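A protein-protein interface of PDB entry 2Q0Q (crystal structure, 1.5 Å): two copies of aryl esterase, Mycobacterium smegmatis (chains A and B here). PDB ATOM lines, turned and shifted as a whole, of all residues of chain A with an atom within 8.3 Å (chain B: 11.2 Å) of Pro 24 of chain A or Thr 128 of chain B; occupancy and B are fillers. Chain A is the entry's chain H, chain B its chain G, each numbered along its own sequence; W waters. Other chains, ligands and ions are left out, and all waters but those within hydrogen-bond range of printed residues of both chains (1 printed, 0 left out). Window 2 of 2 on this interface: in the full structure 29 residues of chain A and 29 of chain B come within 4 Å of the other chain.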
ATOM      1  N   TRP A  14      12.514   9.824 -33.317  1.00  0.00           N
ATOM      2  CA  TRP A  14      12.918  10.193 -31.956  1.00  0.00           C
ATOM      3  C   TRP A  14      12.294   9.257 -30.921  1.00  0.00           C
ATOM      4  O   TRP A  14      12.945   8.864 -29.946  1.00  0.00           O
ATOM      5  CB  TRP A  14      12.492  11.628 -31.674  1.00  0.00           C
ATOM      6  CG  TRP A  14      12.901  12.158 -30.323  1.00  0.00           C
ATOM      7  CD1 TRP A  14      14.140  12.580 -29.975  1.00  0.00           C
ATOM      8  CD2 TRP A  14      12.065  12.367 -29.170  1.00  0.00           C
ATOM      9  NE1 TRP A  14      14.141  13.027 -28.677  1.00  0.00           N
ATOM     10  CE2 TRP A  14      12.880  12.916 -28.157  1.00  0.00           C
ATOM     11  CE3 TRP A  14      10.707  12.163 -28.903  1.00  0.00           C
ATOM     12  CZ2 TRP A  14      12.394  13.235 -26.894  1.00  0.00           C
ATOM     13  CZ3 TRP A  14      10.223  12.485 -27.653  1.00  0.00           C
ATOM     14  CH2 TRP A  14      11.058  13.018 -26.661  1.00  0.00           C
ATOM     15  N   TRP A  16       8.536   9.543 -29.946  1.00  0.00           N
ATOM     16  CA  TRP A  16       7.539  10.285 -29.190  1.00  0.00           C
ATOM     17  C   TRP A  16       6.478   9.329 -28.619  1.00  0.00           C
ATOM     18  O   TRP A  16       5.801   8.582 -29.375  1.00  0.00           O
ATOM     19  CB  TRP A  16       6.906  11.323 -30.127  1.00  0.00           C
ATOM     20  CG  TRP A  16       5.764  12.111 -29.576  1.00  0.00           C
ATOM     21  CD1 TRP A  16       4.561  11.637 -29.196  1.00  0.00           C
ATOM     22  CD2 TRP A  16       5.729  13.530 -29.360  1.00  0.00           C
ATOM     23  NE1 TRP A  16       3.747  12.671 -28.764  1.00  0.00           N
ATOM     24  CE2 TRP A  16       4.444  13.844 -28.860  1.00  0.00           C
ATOM     25  CE3 TRP A  16       6.653  14.569 -29.558  1.00  0.00           C
ATOM     26  CZ2 TRP A  16       4.062  15.156 -28.528  1.00  0.00           C
ATOM     27  CZ3 TRP A  16       6.287  15.866 -29.222  1.00  0.00           C
ATOM     28  CH2 TRP A  16       4.988  16.154 -28.718  1.00  0.00           C
ATOM     29  N   VAL A  17       6.279   9.380 -27.307  1.00  0.00           N
ATOM     30  CA  VAL A  17       5.220   8.556 -26.665  1.00  0.00           C
ATOM     31  C   VAL A  17       3.821   9.202 -26.843  1.00  0.00           C
ATOM     32  O   VAL A  17       3.580  10.279 -26.322  1.00  0.00           O
ATOM     33  CB  VAL A  17       5.521   8.298 -25.174  1.00  0.00           C
ATOM     34  CG1 VAL A  17       4.383   7.493 -24.521  1.00  0.00           C
ATOM     35  CG2 VAL A  17       6.860   7.535 -25.029  1.00  0.00           C
ATOM     36  N   PRO A  18       2.899   8.522 -27.568  1.00  0.00           N
ATOM     37  CA  PRO A  18       1.591   9.163 -27.772  1.00  0.00           C
ATOM     38  C   PRO A  18       0.832   9.335 -26.462  1.00  0.00           C
ATOM     39  O   PRO A  18       0.815   8.405 -25.632  1.00  0.00           O
ATOM     40  CB  PRO A  18       0.860   8.224 -28.745  1.00  0.00           C
ATOM     41  CG  PRO A  18       1.732   7.042 -28.978  1.00  0.00           C
ATOM     42  CD  PRO A  18       3.005   7.207 -28.217  1.00  0.00           C
ATOM     43  N   VAL A  19       0.253  10.515 -26.252  1.00  0.00           N
ATOM     44  CA  VAL A  19      -0.572  10.777 -25.062  1.00  0.00           C
ATOM     45  C   VAL A  19      -1.918  11.369 -25.443  1.00  0.00           C
ATOM     46  O   VAL A  19      -2.034  12.097 -26.439  1.00  0.00           O
ATOM     47  CB  VAL A  19       0.129  11.736 -24.033  1.00  0.00           C
ATOM     48  CG1 VAL A  19       1.302  11.051 -23.378  1.00  0.00           C
ATOM     49  CG2 VAL A  19       0.594  13.042 -24.687  1.00  0.00           C
ATOM     50  N   GLU A  20      -2.931  11.010 -24.659  1.00  0.00           N
ATOM     51  CA  GLU A  20      -4.287  11.459 -24.891  1.00  0.00           C
ATOM     52  C   GLU A  20      -4.396  12.969 -24.840  1.00  0.00           C
ATOM     53  O   GLU A  20      -5.144  13.540 -25.612  1.00  0.00           O
ATOM     54  CB  GLU A  20      -5.259  10.755 -23.921  1.00  0.00           C
ATOM     55  CG  GLU A  20      -5.455   9.280 -24.304  1.00  0.00           C
ATOM     56  CD  GLU A  20      -6.600   8.576 -23.568  1.00  0.00           C
ATOM     57  OE1 GLU A  20      -6.368   8.034 -22.457  1.00  0.00           O
ATOM     58  OE2 GLU A  20      -7.719   8.521 -24.132  1.00  0.00           O
ATOM     59  N   ASP A  21      -3.614  13.629 -23.986  1.00  0.00           N
ATOM     60  CA  ASP A  21      -3.716  15.097 -23.886  1.00  0.00           C
ATOM     61  C   ASP A  21      -2.815  15.866 -24.870  1.00  0.00           C
ATOM     62  O   ASP A  21      -2.657  17.077 -24.757  1.00  0.00           O
ATOM     63  CB  ASP A  21      -3.530  15.591 -22.434  1.00  0.00           C
ATOM     64  CG  ASP A  21      -2.133  15.382 -21.909  1.00  0.00           C
ATOM     65  OD1 ASP A  21      -1.227  15.058 -22.692  1.00  0.00           O
ATOM     66  OD2 ASP A  21      -1.922  15.571 -20.696  1.00  0.00           O
ATOM     67  N   GLY A  22      -2.273  15.148 -25.844  1.00  0.00           N
ATOM     68  CA  GLY A  22      -1.566  15.711 -26.965  1.00  0.00           C
ATOM     69  C   GLY A  22      -0.086  15.896 -26.678  1.00  0.00           C
ATOM     70  O   GLY A  22       0.774  15.292 -27.321  1.00  0.00           O
ATOM     71  N   ALA A  23       0.186  16.767 -25.717  1.00  0.00           N
ATOM     72  CA  ALA A  23       1.535  17.050 -25.287  1.00  0.00           C
ATOM     73  C   ALA A  23       1.464  17.755 -23.932  1.00  0.00           C
ATOM     74  O   ALA A  23       0.425  18.284 -23.550  1.00  0.00           O
ATOM     75  CB  ALA A  23       2.246  17.896 -26.312  1.00  0.00           C
ATOM     76  N   PRO A  24       2.578  17.770 -23.200  1.00  0.00           N
ATOM     77  CA  PRO A  24       3.916  17.242 -23.453  1.00  0.00           C
ATOM     78  C   PRO A  24       4.071  15.739 -23.174  1.00  0.00           C
ATOM     79  O   PRO A  24       3.191  15.104 -22.553  1.00  0.00           O
ATOM     80  CB  PRO A  24       4.770  18.030 -22.457  1.00  0.00           C
ATOM     81  CG  PRO A  24       3.859  18.206 -21.305  1.00  0.00           C
ATOM     82  CD  PRO A  24       2.490  18.440 -21.895  1.00  0.00           C
ATOM     83  N   THR A  25       5.183  15.172 -23.624  1.00  0.00           N
ATOM     84  CA  THR A  25       5.393  13.751 -23.478  1.00  0.00           C
ATOM     85  C   THR A  25       6.866  13.451 -23.229  1.00  0.00           C
ATOM     86  O   THR A  25       7.651  14.370 -22.965  1.00  0.00           O
ATOM     87  CB  THR A  25       4.864  13.003 -24.719  1.00  0.00           C
ATOM     88  OG1 THR A  25       4.791  11.605 -24.453  1.00  0.00           O
ATOM     89  CG2 THR A  25       5.733  13.234 -25.924  1.00  0.00           C
ATOM     90  N   GLU A  26       7.208  12.162 -23.288  1.00  0.00           N
ATOM     91  CA  GLU A  26       8.577  11.680 -23.115  1.00  0.00           C
ATOM     92  C   GLU A  26       8.938  10.766 -24.267  1.00  0.00           C
ATOM     93  O   GLU A  26       8.098  10.504 -25.150  1.00  0.00           O
ATOM     94  CB  GLU A  26       8.709  10.904 -21.811  1.00  0.00           C
ATOM     95  CG  GLU A  26       8.472  11.747 -20.558  1.00  0.00           C
ATOM     96  CD  GLU A  26       6.993  11.964 -20.257  1.00  0.00           C
ATOM     97  OE1 GLU A  26       6.605  13.079 -19.824  1.00  0.00           O
ATOM     98  OE2 GLU A  26       6.227  11.011 -20.425  1.00  0.00           O
ATOM     99  N   ARG A  27      10.195  10.318 -24.254  1.00  0.00           N
ATOM    100  CA  ARG A  27      10.713   9.411 -25.235  1.00  0.00           C
ATOM    101  C   ARG A  27      10.479   7.948 -24.869  1.00  0.00           C
ATOM    102  O   ARG A  27      10.649   7.544 -23.697  1.00  0.00           O
ATOM    103  CB  ARG A  27      12.222   9.656 -25.348  1.00  0.00           C
ATOM    104  CG  ARG A  27      12.810   9.269 -26.641  1.00  0.00           C
ATOM    105  CD  ARG A  27      14.210   9.889 -26.774  1.00  0.00           C
ATOM    106  NE  ARG A  27      14.839   9.451 -28.004  1.00  0.00           N
ATOM    107  CZ  ARG A  27      16.067   9.794 -28.391  1.00  0.00           C
ATOM    108  NH1 ARG A  27      16.832  10.559 -27.623  1.00  0.00           N
ATOM    109  NH2 ARG A  27      16.543   9.329 -29.539  1.00  0.00           N
ATOM    110  N   ALA B  79      17.500  19.321 -29.179  1.00  0.00           N
ATOM    111  CA  ALA B  79      16.120  18.826 -29.155  1.00  0.00           C
ATOM    112  C   ALA B  79      16.014  17.377 -29.680  1.00  0.00           C
ATOM    113  O   ALA B  79      15.099  16.645 -29.315  1.00  0.00           O
ATOM    114  CB  ALA B  79      15.217  19.748 -29.951  1.00  0.00           C
ATOM    115  N   LEU B  82      17.489  15.053 -26.476  1.00  0.00           N
ATOM    116  CA  LEU B  82      16.796  14.967 -25.183  1.00  0.00           C
ATOM    117  C   LEU B  82      16.250  13.563 -24.985  1.00  0.00           C
ATOM    118  O   LEU B  82      15.776  12.948 -25.932  1.00  0.00           O
ATOM    119  CB  LEU B  82      15.663  15.966 -25.026  1.00  0.00           C
ATOM    120  CG  LEU B  82      15.991  17.457 -25.038  1.00  0.00           C
ATOM    121  CD1 LEU B  82      14.746  18.219 -24.696  1.00  0.00           C
ATOM    122  CD2 LEU B  82      17.092  17.839 -24.083  1.00  0.00           C
ATOM    123  N   PRO B  83      16.316  13.053 -23.745  1.00  0.00           N
ATOM    124  CA  PRO B  83      16.800  13.749 -22.538  1.00  0.00           C
ATOM    125  C   PRO B  83      18.325  13.810 -22.449  1.00  0.00           C
ATOM    126  O   PRO B  83      19.010  12.871 -22.868  1.00  0.00           O
ATOM    127  CB  PRO B  83      16.222  12.898 -21.420  1.00  0.00           C
ATOM    128  CG  PRO B  83      16.301  11.517 -21.997  1.00  0.00           C
ATOM    129  CD  PRO B  83      15.851  11.693 -23.423  1.00  0.00           C
ATOM    130  N   LEU B  84      18.834  14.931 -21.938  1.00  0.00           N
ATOM    131  CA  LEU B  84      20.268  15.170 -21.792  1.00  0.00           C
ATOM    132  C   LEU B  84      20.562  15.635 -20.380  1.00  0.00           C
ATOM    133  O   LEU B  84      19.756  16.342 -19.763  1.00  0.00           O
ATOM    134  CB  LEU B  84      20.758  16.234 -22.785  1.00  0.00           C
ATOM    135  CG  LEU B  84      20.846  15.835 -24.265  1.00  0.00           C
ATOM    136  CD1 LEU B  84      21.291  17.049 -25.098  1.00  0.00           C
ATOM    137  CD2 LEU B  84      21.793  14.662 -24.492  1.00  0.00           C
ATOM    138  N   SER B 121      17.165  25.346 -23.307  1.00  0.00           N
ATOM    139  CA  SER B 121      16.737  24.227 -24.149  1.00  0.00           C
ATOM    140  C   SER B 121      15.672  23.319 -23.510  1.00  0.00           C
ATOM    141  O   SER B 121      15.283  22.296 -24.118  1.00  0.00           O
ATOM    142  CB  SER B 121      17.955  23.375 -24.525  1.00  0.00           C
ATOM    143  OG  SER B 121      18.492  22.703 -23.399  1.00  0.00           O
ATOM    144  N   ALA B 122      15.225  23.659 -22.296  1.00  0.00           N
ATOM    145  CA  ALA B 122      14.283  22.808 -21.575  1.00  0.00           C
ATOM    146  C   ALA B 122      13.059  22.500 -22.423  1.00  0.00           C
ATOM    147  O   ALA B 122      12.515  23.390 -23.075  1.00  0.00           O
ATOM    148  CB  ALA B 122      13.853  23.448 -20.289  1.00  0.00           C
ATOM    149  N   GLY B 123      12.634  21.232 -22.376  1.00  0.00           N
ATOM    150  CA  GLY B 123      11.432  20.764 -23.048  1.00  0.00           C
ATOM    151  C   GLY B 123      11.595  20.403 -24.509  1.00  0.00           C
ATOM    152  O   GLY B 123      10.747  19.740 -25.043  1.00  0.00           O
ATOM    153  N   GLY B 124      12.662  20.862 -25.166  1.00  0.00           N
ATOM    154  CA  GLY B 124      12.864  20.627 -26.595  1.00  0.00           C
ATOM    155  C   GLY B 124      11.579  20.854 -27.347  1.00  0.00           C
ATOM    156  O   GLY B 124      10.912  21.873 -27.162  1.00  0.00           O
ATOM    157  N   VAL B 125      11.194  19.874 -28.157  1.00  0.00           N
ATOM    158  CA  VAL B 125       9.916  19.924 -28.875  1.00  0.00           C
ATOM    159  C   VAL B 125       8.891  19.074 -28.117  1.00  0.00           C
ATOM    160  O   VAL B 125       8.915  17.855 -28.200  1.00  0.00           O
ATOM    161  CB  VAL B 125      10.063  19.440 -30.318  1.00  0.00           C
ATOM    162  CG1 VAL B 125       8.706  19.482 -31.050  1.00  0.00           C
ATOM    163  CG2 VAL B 125      11.083  20.298 -31.070  1.00  0.00           C
ATOM    164  N   GLY B 126       8.019  19.731 -27.369  1.00  0.00           N
ATOM    165  CA  GLY B 126       6.877  19.050 -26.735  1.00  0.00           C
ATOM    166  C   GLY B 126       7.188  18.036 -25.645  1.00  0.00           C
ATOM    167  O   GLY B 126       6.345  17.176 -25.375  1.00  0.00           O
ATOM    168  N   THR B 127       8.359  18.124 -24.998  1.00  0.00           N
ATOM    169  CA  THR B 127       8.706  17.169 -23.929  1.00  0.00           C
ATOM    170  C   THR B 127       8.644  17.805 -22.543  1.00  0.00           C
ATOM    171  O   THR B 127       8.593  19.024 -22.396  1.00  0.00           O
ATOM    172  CB  THR B 127      10.090  16.495 -24.086  1.00  0.00           C
ATOM    173  OG1 THR B 127      11.120  17.368 -23.575  1.00  0.00           O
ATOM    174  CG2 THR B 127      10.382  16.137 -25.524  1.00  0.00           C
ATOM    175  N   THR B 128       8.659  16.933 -21.539  1.00  0.00           N
ATOM    176  CA  THR B 128       8.724  17.311 -20.131  1.00  0.00           C
ATOM    177  C   THR B 128      10.155  17.380 -19.607  1.00  0.00           C
ATOM    178  O   THR B 128      10.366  17.548 -18.405  1.00  0.00           O
ATOM    179  CB  THR B 128       7.976  16.237 -19.312  1.00  0.00           C
ATOM    180  OG1 THR B 128       8.504  14.948 -19.664  1.00  0.00           O
ATOM    181  CG2 THR B 128       6.478  16.275 -19.596  1.00  0.00           C
ATOM    182  N   TYR B 129      11.152  17.261 -20.482  1.00  0.00           N
ATOM    183  CA  TYR B 129      12.539  17.117 -20.048  1.00  0.00           C
ATOM    184  C   TYR B 129      13.194  18.448 -19.663  1.00  0.00           C
ATOM    185  O   TYR B 129      12.962  19.477 -20.320  1.00  0.00           O
ATOM    186  CB  TYR B 129      13.365  16.432 -21.157  1.00  0.00           C
ATOM    187  CG  TYR B 129      13.001  14.972 -21.404  1.00  0.00           C
ATOM    188  CD1 TYR B 129      12.792  14.489 -22.687  1.00  0.00           C
ATOM    189  CD2 TYR B 129      12.878  14.078 -20.350  1.00  0.00           C
ATOM    190  CE1 TYR B 129      12.491  13.173 -22.918  1.00  0.00           C
ATOM    191  CE2 TYR B 129      12.577  12.748 -20.573  1.00  0.00           C
ATOM    192  CZ  TYR B 129      12.358  12.309 -21.867  1.00  0.00           C
ATOM    193  OH  TYR B 129      12.081  10.986 -22.077  1.00  0.00           O
ATOM    194  N   PRO B 130      14.045  18.429 -18.612  1.00  0.00           N
ATOM    195  CA  PRO B 130      14.737  19.642 -18.180  1.00  0.00           C
ATOM    196  C   PRO B 130      15.908  19.975 -19.110  1.00  0.00           C
ATOM    197  O   PRO B 130      16.330  19.137 -19.894  1.00  0.00           O
ATOM    198  CB  PRO B 130      15.270  19.257 -16.783  1.00  0.00           C
ATOM    199  CG  PRO B 130      15.447  17.790 -16.861  1.00  0.00           C
ATOM    200  CD  PRO B 130      14.363  17.274 -17.747  1.00  0.00           C
ATOM    201  N   ALA B 131      16.425  21.191 -19.021  1.00  0.00           N
ATOM    202  CA  ALA B 131      17.658  21.512 -19.737  1.00  0.00           C
ATOM    203  C   ALA B 131      18.825  20.727 -19.130  1.00  0.00           C
ATOM    204  O   ALA B 131      18.870  20.524 -17.912  1.00  0.00           O
ATOM    205  CB  ALA B 131      17.935  22.989 -19.682  1.00  0.00           C
ATOM    206  N   PRO B 132      19.773  20.277 -19.976  1.00  0.00           N
ATOM    207  CA  PRO B 132      21.016  19.749 -19.446  1.00  0.00           C
ATOM    208  C   PRO B 132      21.876  20.818 -18.806  1.00  0.00           C
ATOM    209  O   PRO B 132      21.634  21.994 -19.023  1.00  0.00           O
ATOM    210  CB  PRO B 132      21.731  19.214 -20.696  1.00  0.00           C
ATOM    211  CG  PRO B 132      21.151  19.929 -21.833  1.00  0.00           C
ATOM    212  CD  PRO B 132      19.740  20.205 -21.447  1.00  0.00           C
HETATM  213  O   HOH W   1      13.128  15.386 -30.835  1.00  0.00           O
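Water W1 lies within hydrogen-bond range of O of Ala 79 of chain B (2.8 Å) and NE1 of Trp 14 of chain A (3.4 Å).
No position is printed for both chains.
The guanidinium group (NH1) of Arg 27 of chain A lies within hydrogen-bond range of the backbone carbonyl oxygen (O) of Leu 82 of chain B (3.1 Å). The backbone carbonyl oxygen of Leu 82 of chain B is in hydrogen-bond range of the indole nitrogen of Trp 14 of chain A (3.2 Å). OG1 of Thr 128 of chain B lies within hydrogen-bond range of OE1 of Glu 26 of chain A, at 2.7 Å. O of Gly 126 of chain B lies within hydrogen-bond range of N of Thr 25 of chain A (2.9 Å). O of Thr 25 of chain A is in hydrogen-bond range of N of Thr 128 of chain B (3.1 Å). The side-chain hydroxyl (OH) of Tyr 129 of chain B sits at hydrogen-bond distance from the backbone NH (N) of Arg 27 of chain A (3.0 Å).
Hydrophobic or aromatic side chains of chain A within 4 Å of the printed part of chain B: Trp 14, Trp 16 and Pro 24. Among the printed residues, no Asp or Glu carboxylate lies within 4 Å of a Lys or Arg side-chain nitrogen of the other chain.
NE of Arg 27 of chain A sits at hydrogen-bond distance from O of Trp 14 of chain A, 2.8 Å away. The backbone carbonyl oxygen of Glu 26 of chain A sits at hydrogen-bond distance from the backbone NH of Val 17 of chain A, at 3.0 Å. N of Gly 123 of chain B is in hydrogen-bond range of O of Tyr 129 of chain B (2.7 Å). The backbone carbonyl oxygen (O) of Gly 123 of chain B sits at hydrogen-bond distance from the side-chain hydroxyl (OG1) of Thr 127 of chain B (2.8 Å). O of Val 17 of chain A lies within hydrogen-bond range of OG1 of Thr 25 of chain A. OG1 of Thr 127 of chain B sits at hydrogen-bond distance from N of Tyr 129 of chain B, 3.1 Å away.
Among the printed residues, merely in contact across the chains: Trp 14 of chain A with Ala 79 of chain B, Trp 14 of chain A with Thr 127 of chain B, Trp 14 of chain A with Tyr 129 of chain B, Trp 16 of chain A with Val 125 of chain B, Trp 16 of chain A with Gly 126 of chain B, Pro 24 of chain A with Gly 126 of chain B, Pro 24 of chain A with Thr 127 of chain B, Pro 24 of chain A with Thr 128 of chain B, Thr 25 of chain A with Thr 127 of chain B and Glu 26 of chain A with Tyr 129 of chain B.
No residue of chain B comes within 4 Å of Asp 21 of chain A. No residue of chain B comes within 4 Å of Gly 22 of chain A. No residue of chain B comes within 4 Å of Ala 23 of chain A. Pro 24 of chain A touches just these residues of chain B: Gly 126, Thr 127 and Thr 128. Of the printed residues of chain B, Glu 26 of chain A touches Thr 128 (2.7 Å) and Tyr 129 (3.4 Å). Of the printed residues of chain A, Thr 127 of chain B touches Trp 14, Pro 24 and Thr 25. Of chain A, only Pro 24, Thr 25 and Glu 26 come within 4 Å of Thr 128 of chain B. Of the printed residues of chain A, Tyr 129 of chain B touches Trp 14, Glu 26 and Arg 27. The nearest printed residue of chain B that does not touch Pro 24 of chain A is Tyr 129 of chain B (6.7 Å). The nearest printed residue of chain B that does not touch Trp 16 of chain A is Thr 127 of chain B (5.2 Å).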
